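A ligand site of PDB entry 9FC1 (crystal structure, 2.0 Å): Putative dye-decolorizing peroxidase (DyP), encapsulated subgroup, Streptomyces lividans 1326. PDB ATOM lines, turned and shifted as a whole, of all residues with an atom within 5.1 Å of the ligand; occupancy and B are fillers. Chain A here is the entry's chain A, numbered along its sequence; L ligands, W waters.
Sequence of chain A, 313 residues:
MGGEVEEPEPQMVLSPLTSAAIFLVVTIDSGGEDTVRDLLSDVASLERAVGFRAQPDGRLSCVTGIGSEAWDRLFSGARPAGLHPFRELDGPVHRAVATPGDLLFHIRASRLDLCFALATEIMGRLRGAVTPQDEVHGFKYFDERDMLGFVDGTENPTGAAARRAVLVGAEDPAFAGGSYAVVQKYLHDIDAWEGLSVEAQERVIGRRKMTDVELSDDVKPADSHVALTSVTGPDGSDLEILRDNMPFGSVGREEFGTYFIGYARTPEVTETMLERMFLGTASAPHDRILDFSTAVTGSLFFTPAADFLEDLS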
ATOM      1  N   ASP A 146      -7.837  37.179   3.377  1.00  0.00           N
ATOM      2  CA  ASP A 146      -8.938  37.550   4.252  1.00  0.00           C
ATOM      3  C   ASP A 146      -8.634  38.947   4.815  1.00  0.00           C
ATOM      4  O   ASP A 146      -7.630  39.569   4.436  1.00  0.00           O
ATOM      5  CB  ASP A 146      -9.207  36.467   5.292  1.00  0.00           C
ATOM      6  CG  ASP A 146      -8.089  36.118   6.219  1.00  0.00           C
ATOM      7  OD1 ASP A 146      -7.212  37.030   6.448  1.00  0.00           O
ATOM      8  OD2 ASP A 146      -8.045  34.919   6.629  1.00  0.00           O
ATOM      9  N   LEU A 148      -7.518  39.812   7.629  1.00  0.00           N
ATOM     10  CA  LEU A 148      -6.235  39.881   8.358  1.00  0.00           C
ATOM     11  C   LEU A 148      -5.007  39.932   7.439  1.00  0.00           C
ATOM     12  O   LEU A 148      -3.886  40.137   7.917  1.00  0.00           O
ATOM     13  CB  LEU A 148      -6.151  38.669   9.278  1.00  0.00           C
ATOM     14  CG  LEU A 148      -7.288  38.515  10.296  1.00  0.00           C
ATOM     15  CD1 LEU A 148      -7.081  37.265  11.126  1.00  0.00           C
ATOM     16  CD2 LEU A 148      -7.408  39.775  11.148  1.00  0.00           C
ATOM     17  N   PHE A 150      -3.938  37.510   5.383  1.00  0.00           N
ATOM     18  CA  PHE A 150      -3.415  36.184   5.085  1.00  0.00           C
ATOM     19  C   PHE A 150      -4.287  35.480   4.031  1.00  0.00           C
ATOM     20  O   PHE A 150      -5.507  35.599   4.020  1.00  0.00           O
ATOM     21  CB  PHE A 150      -3.345  35.326   6.345  1.00  0.00           C
ATOM     22  CG  PHE A 150      -2.201  35.688   7.258  1.00  0.00           C
ATOM     23  CD1 PHE A 150      -2.161  36.928   7.903  1.00  0.00           C
ATOM     24  CD2 PHE A 150      -1.116  34.847   7.369  1.00  0.00           C
ATOM     25  CE1 PHE A 150      -1.068  37.298   8.685  1.00  0.00           C
ATOM     26  CE2 PHE A 150      -0.045  35.218   8.147  1.00  0.00           C
ATOM     27  CZ  PHE A 150      -0.002  36.436   8.797  1.00  0.00           C
ATOM     28  N   VAL A 151      -3.612  34.694   3.180  1.00  0.00           N
ATOM     29  CA  VAL A 151      -4.288  33.815   2.239  1.00  0.00           C
ATOM     30  C   VAL A 151      -5.133  32.835   3.036  1.00  0.00           C
ATOM     31  O   VAL A 151      -4.696  32.309   4.046  1.00  0.00           O
ATOM     32  CB  VAL A 151      -3.293  33.072   1.316  1.00  0.00           C
ATOM     33  CG1 VAL A 151      -3.989  32.162   0.331  1.00  0.00           C
ATOM     34  CG2 VAL A 151      -2.426  34.032   0.518  1.00  0.00           C
ATOM     35  N   ASP A 152      -6.355  32.624   2.534  1.00  0.00           N
ATOM     36  CA  ASP A 152      -7.396  31.898   3.279  1.00  0.00           C
ATOM     37  C   ASP A 152      -8.015  30.840   2.366  1.00  0.00           C
ATOM     38  O   ASP A 152      -8.623  31.187   1.360  1.00  0.00           O
ATOM     39  CB  ASP A 152      -8.419  32.923   3.811  1.00  0.00           C
ATOM     40  CG  ASP A 152      -9.319  32.378   4.903  1.00  0.00           C
ATOM     41  OD1 ASP A 152      -9.773  31.230   4.722  1.00  0.00           O
ATOM     42  OD2 ASP A 152      -9.545  33.093   5.937  1.00  0.00           O
ATOM     43  N   GLY A 153      -7.810  29.550   2.693  1.00  0.00           N
ATOM     44  CA  GLY A 153      -8.346  28.392   1.956  1.00  0.00           C
ATOM     45  C   GLY A 153      -7.291  27.403   1.400  1.00  0.00           C
ATOM     46  O   GLY A 153      -7.632  26.318   0.950  1.00  0.00           O
ATOM     47  N   THR A 154      -6.001  27.725   1.603  1.00  0.00           N
ATOM     48  CA  THR A 154      -4.900  26.997   1.036  1.00  0.00           C
ATOM     49  C   THR A 154      -4.952  25.506   1.316  1.00  0.00           C
ATOM     50  O   THR A 154      -4.763  24.726   0.387  1.00  0.00           O
ATOM     51  CB  THR A 154      -3.590  27.558   1.586  1.00  0.00           C
ATOM     52  OG1 THR A 154      -3.606  28.975   1.441  1.00  0.00           O
ATOM     53  CG2 THR A 154      -2.418  27.026   0.792  1.00  0.00           C
ATOM     54  N   GLU A 155      -5.162  25.082   2.578  1.00  0.00           N
ATOM     55  CA  GLU A 155      -5.092  23.678   2.945  1.00  0.00           C
ATOM     56  C   GLU A 155      -6.461  22.992   2.891  1.00  0.00           C
ATOM     57  O   GLU A 155      -6.611  21.875   3.414  1.00  0.00           O
ATOM     58  CB  GLU A 155      -4.448  23.482   4.326  1.00  0.00           C
ATOM     59  CG  GLU A 155      -2.944  23.717   4.345  1.00  0.00           C
ATOM     60  CD  GLU A 155      -2.164  22.815   3.424  1.00  0.00           C
ATOM     61  OE1 GLU A 155      -2.271  21.633   3.650  1.00  0.00           O
ATOM     62  OE2 GLU A 155      -1.535  23.304   2.460  1.00  0.00           O
ATOM     63  N   ASN A 156      -7.469  23.591   2.231  1.00  0.00           N
ATOM     64  CA  ASN A 156      -8.682  22.833   2.014  1.00  0.00           C
ATOM     65  C   ASN A 156      -8.367  21.521   1.271  1.00  0.00           C
ATOM     66  O   ASN A 156      -7.553  21.512   0.353  1.00  0.00           O
ATOM     67  CB  ASN A 156      -9.697  23.626   1.216  1.00  0.00           C
ATOM     68  CG  ASN A 156     -10.632  24.471   2.056  1.00  0.00           C
ATOM     69  OD1 ASN A 156     -11.026  24.103   3.143  1.00  0.00           O
ATOM     70  ND2 ASN A 156     -11.037  25.623   1.549  1.00  0.00           N
ATOM     71  N   GLN A 184     -20.223  30.865  11.574  1.00  0.00           N
ATOM     72  CA  GLN A 184     -19.956  31.852  12.585  1.00  0.00           C
ATOM     73  C   GLN A 184     -19.524  33.145  11.904  1.00  0.00           C
ATOM     74  O   GLN A 184     -18.578  33.189  11.126  1.00  0.00           O
ATOM     75  CB  GLN A 184     -18.820  31.413  13.508  1.00  0.00           C
ATOM     76  CG  GLN A 184     -19.035  30.157  14.364  1.00  0.00           C
ATOM     77  CD  GLN A 184     -17.764  29.941  15.174  1.00  0.00           C
ATOM     78  OE1 GLN A 184     -16.673  29.685  14.649  1.00  0.00           O
ATOM     79  NE2 GLN A 184     -17.873  30.185  16.486  1.00  0.00           N
ATOM     80  N   TYR A 186     -17.557  36.418  12.322  1.00  0.00           N
ATOM     81  CA  TYR A 186     -16.523  37.058  13.128  1.00  0.00           C
ATOM     82  C   TYR A 186     -16.290  38.513  12.707  1.00  0.00           C
ATOM     83  O   TYR A 186     -16.279  38.824  11.516  1.00  0.00           O
ATOM     84  CB  TYR A 186     -15.191  36.313  12.976  1.00  0.00           C
ATOM     85  CG  TYR A 186     -15.088  34.986  13.682  1.00  0.00           C
ATOM     86  CD1 TYR A 186     -14.672  34.892  14.998  1.00  0.00           C
ATOM     87  CD2 TYR A 186     -15.429  33.813  13.030  1.00  0.00           C
ATOM     88  CE1 TYR A 186     -14.547  33.654  15.630  1.00  0.00           C
ATOM     89  CE2 TYR A 186     -15.380  32.595  13.659  1.00  0.00           C
ATOM     90  CZ  TYR A 186     -14.869  32.500  14.944  1.00  0.00           C
ATOM     91  OH  TYR A 186     -14.836  31.285  15.557  1.00  0.00           O
ATOM     92  N   HIS A 188     -13.359  41.512  13.388  1.00  0.00           N
ATOM     93  CA  HIS A 188     -11.971  41.635  13.753  1.00  0.00           C
ATOM     94  C   HIS A 188     -11.689  42.999  14.369  1.00  0.00           C
ATOM     95  O   HIS A 188     -12.245  43.987  13.938  1.00  0.00           O
ATOM     96  CB  HIS A 188     -11.064  41.395  12.550  1.00  0.00           C
ATOM     97  CG  HIS A 188     -11.233  40.021  11.992  1.00  0.00           C
ATOM     98  ND1 HIS A 188     -10.770  38.932  12.677  1.00  0.00           N
ATOM     99  CD2 HIS A 188     -11.695  39.578  10.777  1.00  0.00           C
ATOM    100  CE1 HIS A 188     -11.082  37.858  11.909  1.00  0.00           C
ATOM    101  NE2 HIS A 188     -11.579  38.248  10.727  1.00  0.00           N
ATOM    102  N   ILE A 205      -0.987  32.974  13.247  1.00  0.00           N
ATOM    103  CA  ILE A 205      -1.656  32.177  12.214  1.00  0.00           C
ATOM    104  C   ILE A 205      -0.961  30.816  12.090  1.00  0.00           C
ATOM    105  O   ILE A 205      -1.628  29.785  12.003  1.00  0.00           O
ATOM    106  CB  ILE A 205      -1.703  32.925  10.859  1.00  0.00           C
ATOM    107  CG1 ILE A 205      -2.443  34.266  10.930  1.00  0.00           C
ATOM    108  CG2 ILE A 205      -2.244  32.039   9.734  1.00  0.00           C
ATOM    109  CD1 ILE A 205      -3.883  34.172  11.200  1.00  0.00           C
ATOM    110  N   ARG A 207       1.629  30.553   9.439  1.00  0.00           N
ATOM    111  CA  ARG A 207       2.115  30.548   8.059  1.00  0.00           C
ATOM    112  C   ARG A 207       2.738  31.925   7.796  1.00  0.00           C
ATOM    113  O   ARG A 207       2.409  32.879   8.486  1.00  0.00           O
ATOM    114  CB  ARG A 207       0.974  30.319   7.056  1.00  0.00           C
ATOM    115  CG  ARG A 207       0.106  29.083   7.353  1.00  0.00           C
ATOM    116  CD  ARG A 207      -1.006  28.847   6.339  1.00  0.00           C
ATOM    117  NE  ARG A 207      -0.474  28.422   5.055  1.00  0.00           N
ATOM    118  CZ  ARG A 207      -0.229  27.150   4.719  1.00  0.00           C
ATOM    119  NH1 ARG A 207      -0.620  26.157   5.485  1.00  0.00           N
ATOM    120  NH2 ARG A 207       0.352  26.889   3.574  1.00  0.00           N
ATOM    121  N   ASP A 212       2.781  32.464   2.117  1.00  0.00           N
ATOM    122  CA  ASP A 212       1.803  31.463   2.501  1.00  0.00           C
ATOM    123  C   ASP A 212       2.463  30.092   2.643  1.00  0.00           C
ATOM    124  O   ASP A 212       1.791  29.074   2.539  1.00  0.00           O
ATOM    125  CB  ASP A 212       0.669  31.349   1.488  1.00  0.00           C
ATOM    126  CG  ASP A 212      -0.559  30.612   1.990  1.00  0.00           C
ATOM    127  OD1 ASP A 212      -0.731  30.533   3.273  1.00  0.00           O
ATOM    128  OD2 ASP A 212      -1.331  30.158   1.065  1.00  0.00           O
ATOM    129  N   HIS A 225      -3.125  29.275  15.055  1.00  0.00           N
ATOM    130  CA  HIS A 225      -4.360  28.832  14.442  1.00  0.00           C
ATOM    131  C   HIS A 225      -4.210  27.488  13.734  1.00  0.00           C
ATOM    132  O   HIS A 225      -5.042  26.564  13.928  1.00  0.00           O
ATOM    133  CB  HIS A 225      -4.889  29.906  13.496  1.00  0.00           C
ATOM    134  CG  HIS A 225      -6.174  29.582  12.894  1.00  0.00           C
ATOM    135  ND1 HIS A 225      -7.284  29.343  13.659  1.00  0.00           N
ATOM    136  CD2 HIS A 225      -6.566  29.555  11.619  1.00  0.00           C
ATOM    137  CE1 HIS A 225      -8.305  29.046  12.828  1.00  0.00           C
ATOM    138  NE2 HIS A 225      -7.923  29.219  11.606  1.00  0.00           N
ATOM    139  N   VAL A 226      -3.165  27.387  12.926  1.00  0.00           N
ATOM    140  CA  VAL A 226      -2.931  26.175  12.188  1.00  0.00           C
ATOM    141  C   VAL A 226      -2.640  24.981  13.141  1.00  0.00           C
ATOM    142  O   VAL A 226      -3.009  23.856  12.863  1.00  0.00           O
ATOM    143  CB  VAL A 226      -1.814  26.373  11.153  1.00  0.00           C
ATOM    144  CG1 VAL A 226      -1.304  25.053  10.603  1.00  0.00           C
ATOM    145  CG2 VAL A 226      -2.282  27.229  10.000  1.00  0.00           C
ATOM    146  N   THR A 229      -6.004  23.778  14.764  1.00  0.00           N
ATOM    147  CA  THR A 229      -7.033  23.268  13.877  1.00  0.00           C
ATOM    148  C   THR A 229      -6.541  22.070  13.059  1.00  0.00           C
ATOM    149  O   THR A 229      -7.269  21.599  12.170  1.00  0.00           O
ATOM    150  CB  THR A 229      -7.615  24.382  12.978  1.00  0.00           C
ATOM    151  OG1 THR A 229      -6.589  24.976  12.178  1.00  0.00           O
ATOM    152  CG2 THR A 229      -8.310  25.449  13.811  1.00  0.00           C
ATOM    153  N   SER A 230      -5.302  21.640  13.318  1.00  0.00           N
ATOM    154  CA  SER A 230      -4.775  20.383  12.808  1.00  0.00           C
ATOM    155  C   SER A 230      -5.121  19.250  13.787  1.00  0.00           C
ATOM    156  O   SER A 230      -4.686  19.327  14.941  1.00  0.00           O
ATOM    157  CB  SER A 230      -3.283  20.456  12.634  1.00  0.00           C
ATOM    158  OG  SER A 230      -2.979  21.451  11.714  1.00  0.00           O
ATOM    159  N   ILE A 241     -11.963  19.445   7.219  1.00  0.00           N
ATOM    160  CA  ILE A 241     -13.197  20.109   6.838  1.00  0.00           C
ATOM    161  C   ILE A 241     -12.944  20.939   5.598  1.00  0.00           C
ATOM    162  O   ILE A 241     -11.824  21.197   5.252  1.00  0.00           O
ATOM    163  CB  ILE A 241     -13.743  20.979   7.967  1.00  0.00           C
ATOM    164  CG1 ILE A 241     -12.872  22.209   8.236  1.00  0.00           C
ATOM    165  CG2 ILE A 241     -14.002  20.126   9.215  1.00  0.00           C
ATOM    166  CD1 ILE A 241     -13.515  23.147   9.238  1.00  0.00           C
ATOM    167  N   ARG A 243     -13.754  24.581   3.975  1.00  0.00           N
ATOM    168  CA  ARG A 243     -14.101  25.956   4.388  1.00  0.00           C
ATOM    169  C   ARG A 243     -14.272  26.829   3.143  1.00  0.00           C
ATOM    170  O   ARG A 243     -13.644  26.563   2.121  1.00  0.00           O
ATOM    171  CB  ARG A 243     -12.988  26.559   5.235  1.00  0.00           C
ATOM    172  CG  ARG A 243     -12.779  25.836   6.544  1.00  0.00           C
ATOM    173  CD  ARG A 243     -11.508  26.298   7.213  1.00  0.00           C
ATOM    174  NE  ARG A 243     -10.378  25.757   6.452  1.00  0.00           N
ATOM    175  CZ  ARG A 243      -9.370  26.461   5.939  1.00  0.00           C
ATOM    176  NH1 ARG A 243      -9.303  27.770   6.141  1.00  0.00           N
ATOM    177  NH2 ARG A 243      -8.420  25.845   5.220  1.00  0.00           N
ATOM    178  N   ASN A 245     -14.572  30.601   3.669  1.00  0.00           N
ATOM    179  CA  ASN A 245     -14.572  31.878   4.368  1.00  0.00           C
ATOM    180  C   ASN A 245     -14.649  33.083   3.434  1.00  0.00           C
ATOM    181  O   ASN A 245     -13.963  33.133   2.420  1.00  0.00           O
ATOM    182  CB  ASN A 245     -13.335  32.008   5.276  1.00  0.00           C
ATOM    183  CG  ASN A 245     -13.254  30.929   6.333  1.00  0.00           C
ATOM    184  OD1 ASN A 245     -14.194  30.149   6.561  1.00  0.00           O
ATOM    185  ND2 ASN A 245     -12.097  30.770   6.924  1.00  0.00           N
ATOM    186  N   THR A 258     -14.848  38.369   8.960  1.00  0.00           N
ATOM    187  CA  THR A 258     -14.744  37.111   8.232  1.00  0.00           C
ATOM    188  C   THR A 258     -15.992  36.285   8.538  1.00  0.00           C
ATOM    189  O   THR A 258     -16.310  36.044   9.704  1.00  0.00           O
ATOM    190  CB  THR A 258     -13.517  36.313   8.618  1.00  0.00           C
ATOM    191  OG1 THR A 258     -12.329  37.037   8.395  1.00  0.00           O
ATOM    192  CG2 THR A 258     -13.411  34.980   7.905  1.00  0.00           C
ATOM    193  N   PHE A 260     -17.257  32.742   8.522  1.00  0.00           N
ATOM    194  CA  PHE A 260     -16.753  31.399   8.570  1.00  0.00           C
ATOM    195  C   PHE A 260     -17.886  30.430   8.206  1.00  0.00           C
ATOM    196  O   PHE A 260     -18.947  30.493   8.775  1.00  0.00           O
ATOM    197  CB  PHE A 260     -16.195  31.025   9.961  1.00  0.00           C
ATOM    198  CG  PHE A 260     -15.881  29.563  10.108  1.00  0.00           C
ATOM    199  CD1 PHE A 260     -14.728  29.028   9.598  1.00  0.00           C
ATOM    200  CD2 PHE A 260     -16.806  28.705  10.678  1.00  0.00           C
ATOM    201  CE1 PHE A 260     -14.503  27.656   9.654  1.00  0.00           C
ATOM    202  CE2 PHE A 260     -16.558  27.333  10.737  1.00  0.00           C
ATOM    203  CZ  PHE A 260     -15.396  26.821  10.263  1.00  0.00           C
ATOM    204  N   THR A 270     -15.812  19.326  13.194  1.00  0.00           N
ATOM    205  CA  THR A 270     -15.860  20.764  13.364  1.00  0.00           C
ATOM    206  C   THR A 270     -15.887  21.180  14.827  1.00  0.00           C
ATOM    207  O   THR A 270     -15.217  22.142  15.220  1.00  0.00           O
ATOM    208  CB  THR A 270     -17.056  21.361  12.603  1.00  0.00           C
ATOM    209  OG1 THR A 270     -17.119  20.825  11.293  1.00  0.00           O
ATOM    210  CG2 THR A 270     -16.918  22.861  12.469  1.00  0.00           C
ATOM    211  N   MET A 273     -12.484  20.884  16.566  1.00  0.00           N
ATOM    212  CA  MET A 273     -11.662  22.044  16.234  1.00  0.00           C
ATOM    213  C   MET A 273     -12.078  23.269  17.033  1.00  0.00           C
ATOM    214  O   MET A 273     -11.220  23.973  17.588  1.00  0.00           O
ATOM    215  CB  MET A 273     -11.762  22.359  14.747  1.00  0.00           C
ATOM    216  CG  MET A 273     -11.066  21.345  13.861  1.00  0.00           C
ATOM    217  SD  MET A 273     -11.417  21.686  12.139  1.00  0.00           S
ATOM    218  CE  MET A 273     -10.489  20.371  11.380  1.00  0.00           C
ATOM    219  N   LEU A 274     -13.395  23.545  17.131  1.00  0.00           N
ATOM    220  CA  LEU A 274     -13.888  24.677  17.924  1.00  0.00           C
ATOM    221  C   LEU A 274     -13.516  24.537  19.394  1.00  0.00           C
ATOM    222  O   LEU A 274     -13.196  25.540  20.026  1.00  0.00           O
ATOM    223  CB  LEU A 274     -15.405  24.803  17.763  1.00  0.00           C
ATOM    224  CG  LEU A 274     -15.864  25.414  16.424  1.00  0.00           C
ATOM    225  CD1 LEU A 274     -17.370  25.274  16.255  1.00  0.00           C
ATOM    226  CD2 LEU A 274     -15.499  26.904  16.312  1.00  0.00           C
ATOM    227  N   MET A 277      -9.950  25.535  19.873  1.00  0.00           N
ATOM    228  CA  MET A 277      -9.766  26.974  19.700  1.00  0.00           C
ATOM    229  C   MET A 277     -10.231  27.760  20.934  1.00  0.00           C
ATOM    230  O   MET A 277      -9.535  28.701  21.335  1.00  0.00           O
ATOM    231  CB  MET A 277     -10.533  27.484  18.459  1.00  0.00           C
ATOM    232  CG  MET A 277      -9.957  27.025  17.100  1.00  0.00           C
ATOM    233  SD  MET A 277     -11.031  27.570  15.719  1.00  0.00           S
ATOM    234  CE  MET A 277     -11.051  29.345  15.944  1.00  0.00           C
ATOM    235  N   ILE A 289      -5.777  33.550  17.285  1.00  0.00           N
ATOM    236  CA  ILE A 289      -6.609  34.306  16.355  1.00  0.00           C
ATOM    237  C   ILE A 289      -7.791  34.955  17.081  1.00  0.00           C
ATOM    238  O   ILE A 289      -8.256  36.005  16.656  1.00  0.00           O
ATOM    239  CB  ILE A 289      -7.026  33.455  15.133  1.00  0.00           C
ATOM    240  CG1 ILE A 289      -7.272  34.299  13.874  1.00  0.00           C
ATOM    241  CG2 ILE A 289      -8.247  32.641  15.390  1.00  0.00           C
ATOM    242  CD1 ILE A 289      -7.432  33.482  12.576  1.00  0.00           C
ATOM    243  N   SER A 293     -10.430  38.533  17.094  1.00  0.00           N
ATOM    244  CA  SER A 293     -11.591  38.028  16.359  1.00  0.00           C
ATOM    245  C   SER A 293     -12.679  37.642  17.364  1.00  0.00           C
ATOM    246  O   SER A 293     -12.463  36.761  18.196  1.00  0.00           O
ATOM    247  CB  SER A 293     -11.241  36.837  15.491  1.00  0.00           C
ATOM    248  OG  SER A 293     -10.126  37.089  14.673  1.00  0.00           O
HETATM  249  C1  LIG L   1      -6.599  27.573   8.233  1.00  0.00           C
HETATM  250  C2  LIG L   1      -8.178  32.064   8.803  1.00  0.00           C
HETATM  251  C3  LIG L   1     -11.772  30.491  11.673  1.00  0.00           C
HETATM  252  C4  LIG L   1     -10.405  26.078  10.738  1.00  0.00           C
HETATM  253  C5  LIG L   1      -6.682  28.941   8.163  1.00  0.00           C
HETATM  254  C6  LIG L   1      -5.741  29.816   7.516  1.00  0.00           C
HETATM  255  C7  LIG L   1      -6.234  31.067   7.648  1.00  0.00           C
HETATM  256  C8  LIG L   1      -7.423  31.010   8.415  1.00  0.00           C
HETATM  257  C9  LIG L   1      -5.617  32.344   7.193  1.00  0.00           C
HETATM  258  C10 LIG L   1      -4.484  29.406   6.829  1.00  0.00           C
HETATM  259  C11 LIG L   1      -4.617  29.098   5.323  1.00  0.00           C
HETATM  260  C12 LIG L   1      -5.610  27.992   5.034  1.00  0.00           C
HETATM  261  O1  LIG L   1      -6.808  28.317   5.019  1.00  0.00           O
HETATM  262  O2  LIG L   1      -5.256  26.795   5.012  1.00  0.00           O
HETATM  263  C13 LIG L   1      -9.300  32.009   9.656  1.00  0.00           C
HETATM  264  C14 LIG L   1      -9.957  33.171  10.122  1.00  0.00           C
HETATM  265  C15 LIG L   1     -11.020  32.794  10.864  1.00  0.00           C
HETATM  266  C16 LIG L   1     -10.920  31.328  10.961  1.00  0.00           C
HETATM  267  C17 LIG L   1      -9.678  34.610   9.639  1.00  0.00           C
HETATM  268  C18 LIG L   1     -11.788  33.833  11.585  1.00  0.00           C
HETATM  269  C19 LIG L   1     -11.916  33.744  12.873  1.00  0.00           C
HETATM  270  C20 LIG L   1     -11.766  29.143  11.740  1.00  0.00           C
HETATM  271  C21 LIG L   1     -12.677  28.237  12.478  1.00  0.00           C
HETATM  272  C22 LIG L   1     -12.206  26.990  12.236  1.00  0.00           C
HETATM  273  C23 LIG L   1     -11.070  27.123  11.352  1.00  0.00           C
HETATM  274  C24 LIG L   1     -13.837  28.688  13.358  1.00  0.00           C
HETATM  275  C25 LIG L   1     -12.634  25.665  12.608  1.00  0.00           C
HETATM  276  C26 LIG L   1     -13.560  25.357  13.375  1.00  0.00           C
HETATM  277  C27 LIG L   1      -9.288  26.176   9.917  1.00  0.00           C
HETATM  278  C28 LIG L   1      -8.649  25.010   9.424  1.00  0.00           C
HETATM  279  C29 LIG L   1      -7.525  25.370   8.809  1.00  0.00           C
HETATM  280  C30 LIG L   1      -7.559  26.817   8.891  1.00  0.00           C
HETATM  281  C31 LIG L   1      -9.033  23.636   9.611  1.00  0.00           C
HETATM  282  C32 LIG L   1      -6.544  24.465   8.102  1.00  0.00           C
HETATM  283  C33 LIG L   1      -5.415  24.049   9.011  1.00  0.00           C
HETATM  284  C34 LIG L   1      -4.415  23.047   8.373  1.00  0.00           C
HETATM  285  O3  LIG L   1      -4.706  21.866   8.443  1.00  0.00           O
HETATM  286  O4  LIG L   1      -3.419  23.375   7.706  1.00  0.00           O
HETATM  287  N1  LIG L   1      -7.680  29.694   8.767  1.00  0.00           N
HETATM  288  N2  LIG L   1      -9.873  30.995  10.229  1.00  0.00           N
HETATM  289  N3  LIG L   1     -10.837  28.438  11.094  1.00  0.00           N
HETATM  290  N4  LIG L   1      -8.622  27.246   9.562  1.00  0.00           N
HETATM  291 FE1  LIG L   1      -9.249  29.069   9.874  1.00  0.00          FE
HETATM  292  O   HOH W   1      -3.166  25.991   6.868  1.00  0.00           O
HETATM  293  O   HOH W   2      -6.853  20.948   9.426  1.00  0.00           O
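N of Gly 153 lies within hydrogen-bond range of O1 of the ligand.
FE1 of the ligand is bound by NE2 of His 225, at 2.2 Å.
N of Glu 155 sits at hydrogen-bond distance from O2 of the ligand, at 3.0 Å.
The guanidinium group of Arg 243 lies within salt-bridge range of an oxygen (O1) of the ligand.
O of Val 226 is in hydrogen-bond range of OG of Ser 230 (2.7 Å).
The backbone carbonyl oxygen (O) of Arg 243 sits at hydrogen-bond distance from the side-chain amide nitrogen (ND2) of Asn 156.
OE1 of Gln 184 lies within hydrogen-bond range of OH of Tyr 186 (2.6 Å).
The backbone NH (N) of Leu 148 sits at hydrogen-bond distance from the side-chain carboxylate (OD1) of Asp 146 (3.0 Å).
N of His 225 is in hydrogen-bond range of O of Ile 205 (3.4 Å).
O of Thr 258 sits at hydrogen-bond distance from N of Tyr 186.
The backbone NH of Phe 150 is in hydrogen-bond range of the side-chain carboxylate of Asp 146, 3.5 Å away.
The side-chain hydroxyl (OG1) of Thr 154 is in hydrogen-bond range of the side-chain carboxylate (OD2) of Asp 212, at 2.6 Å.
Asp 146 touches the ligand.
Phe 150 touches the ligand (CB to C9, 3.8 Å).
Val 151 touches the ligand (O to C9, 3.3 Å).
Asp 152 touches the ligand (OD2 to C2, 3.3 Å).
Thr 154 touches the ligand (N to C12, 3.5 Å).
OE1 of Gln 184 touches C24 of the ligand, 3.3 Å away.
CG of Tyr 186 touches C19 of the ligand (3.5 Å).
Arg 207 touches the ligand (CD to C10, 3.6 Å).
Val 226 touches the ligand.
Thr 229 touches the ligand (OG1 to C28, 3.4 Å).
Ser 230 touches the ligand (OG to O3, 3.7 Å).
Asn 245 touches the ligand (ND2 to N2, 3.99 Å).
OG1 of Thr 258 touches C17 of the ligand, 3.8 Å away.
Phe 260 touches the ligand (CE1 to C21, 3.4 Å).
Met 273 touches the ligand.
CG of Leu 274 touches C26 of the ligand, at 3.8 Å.
SD of Met 277 touches C21 of the ligand (3.7 Å).
Ile 289 touches the ligand.
Hydrophobic or aromatic side chains that line the ligand: Phe 150, Tyr 186, His 225, Val 226, Phe 260, Met 273, Leu 274, Met 277 and Ile 289.
Water W2 lies within hydrogen-bond range of O3 of the ligand (2.5 Å) and O of Thr 229 (2.9 Å).
Water W1 bridges O4 of the ligand (2.8 Å) and NH1 of Arg 207 (2.9 Å).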
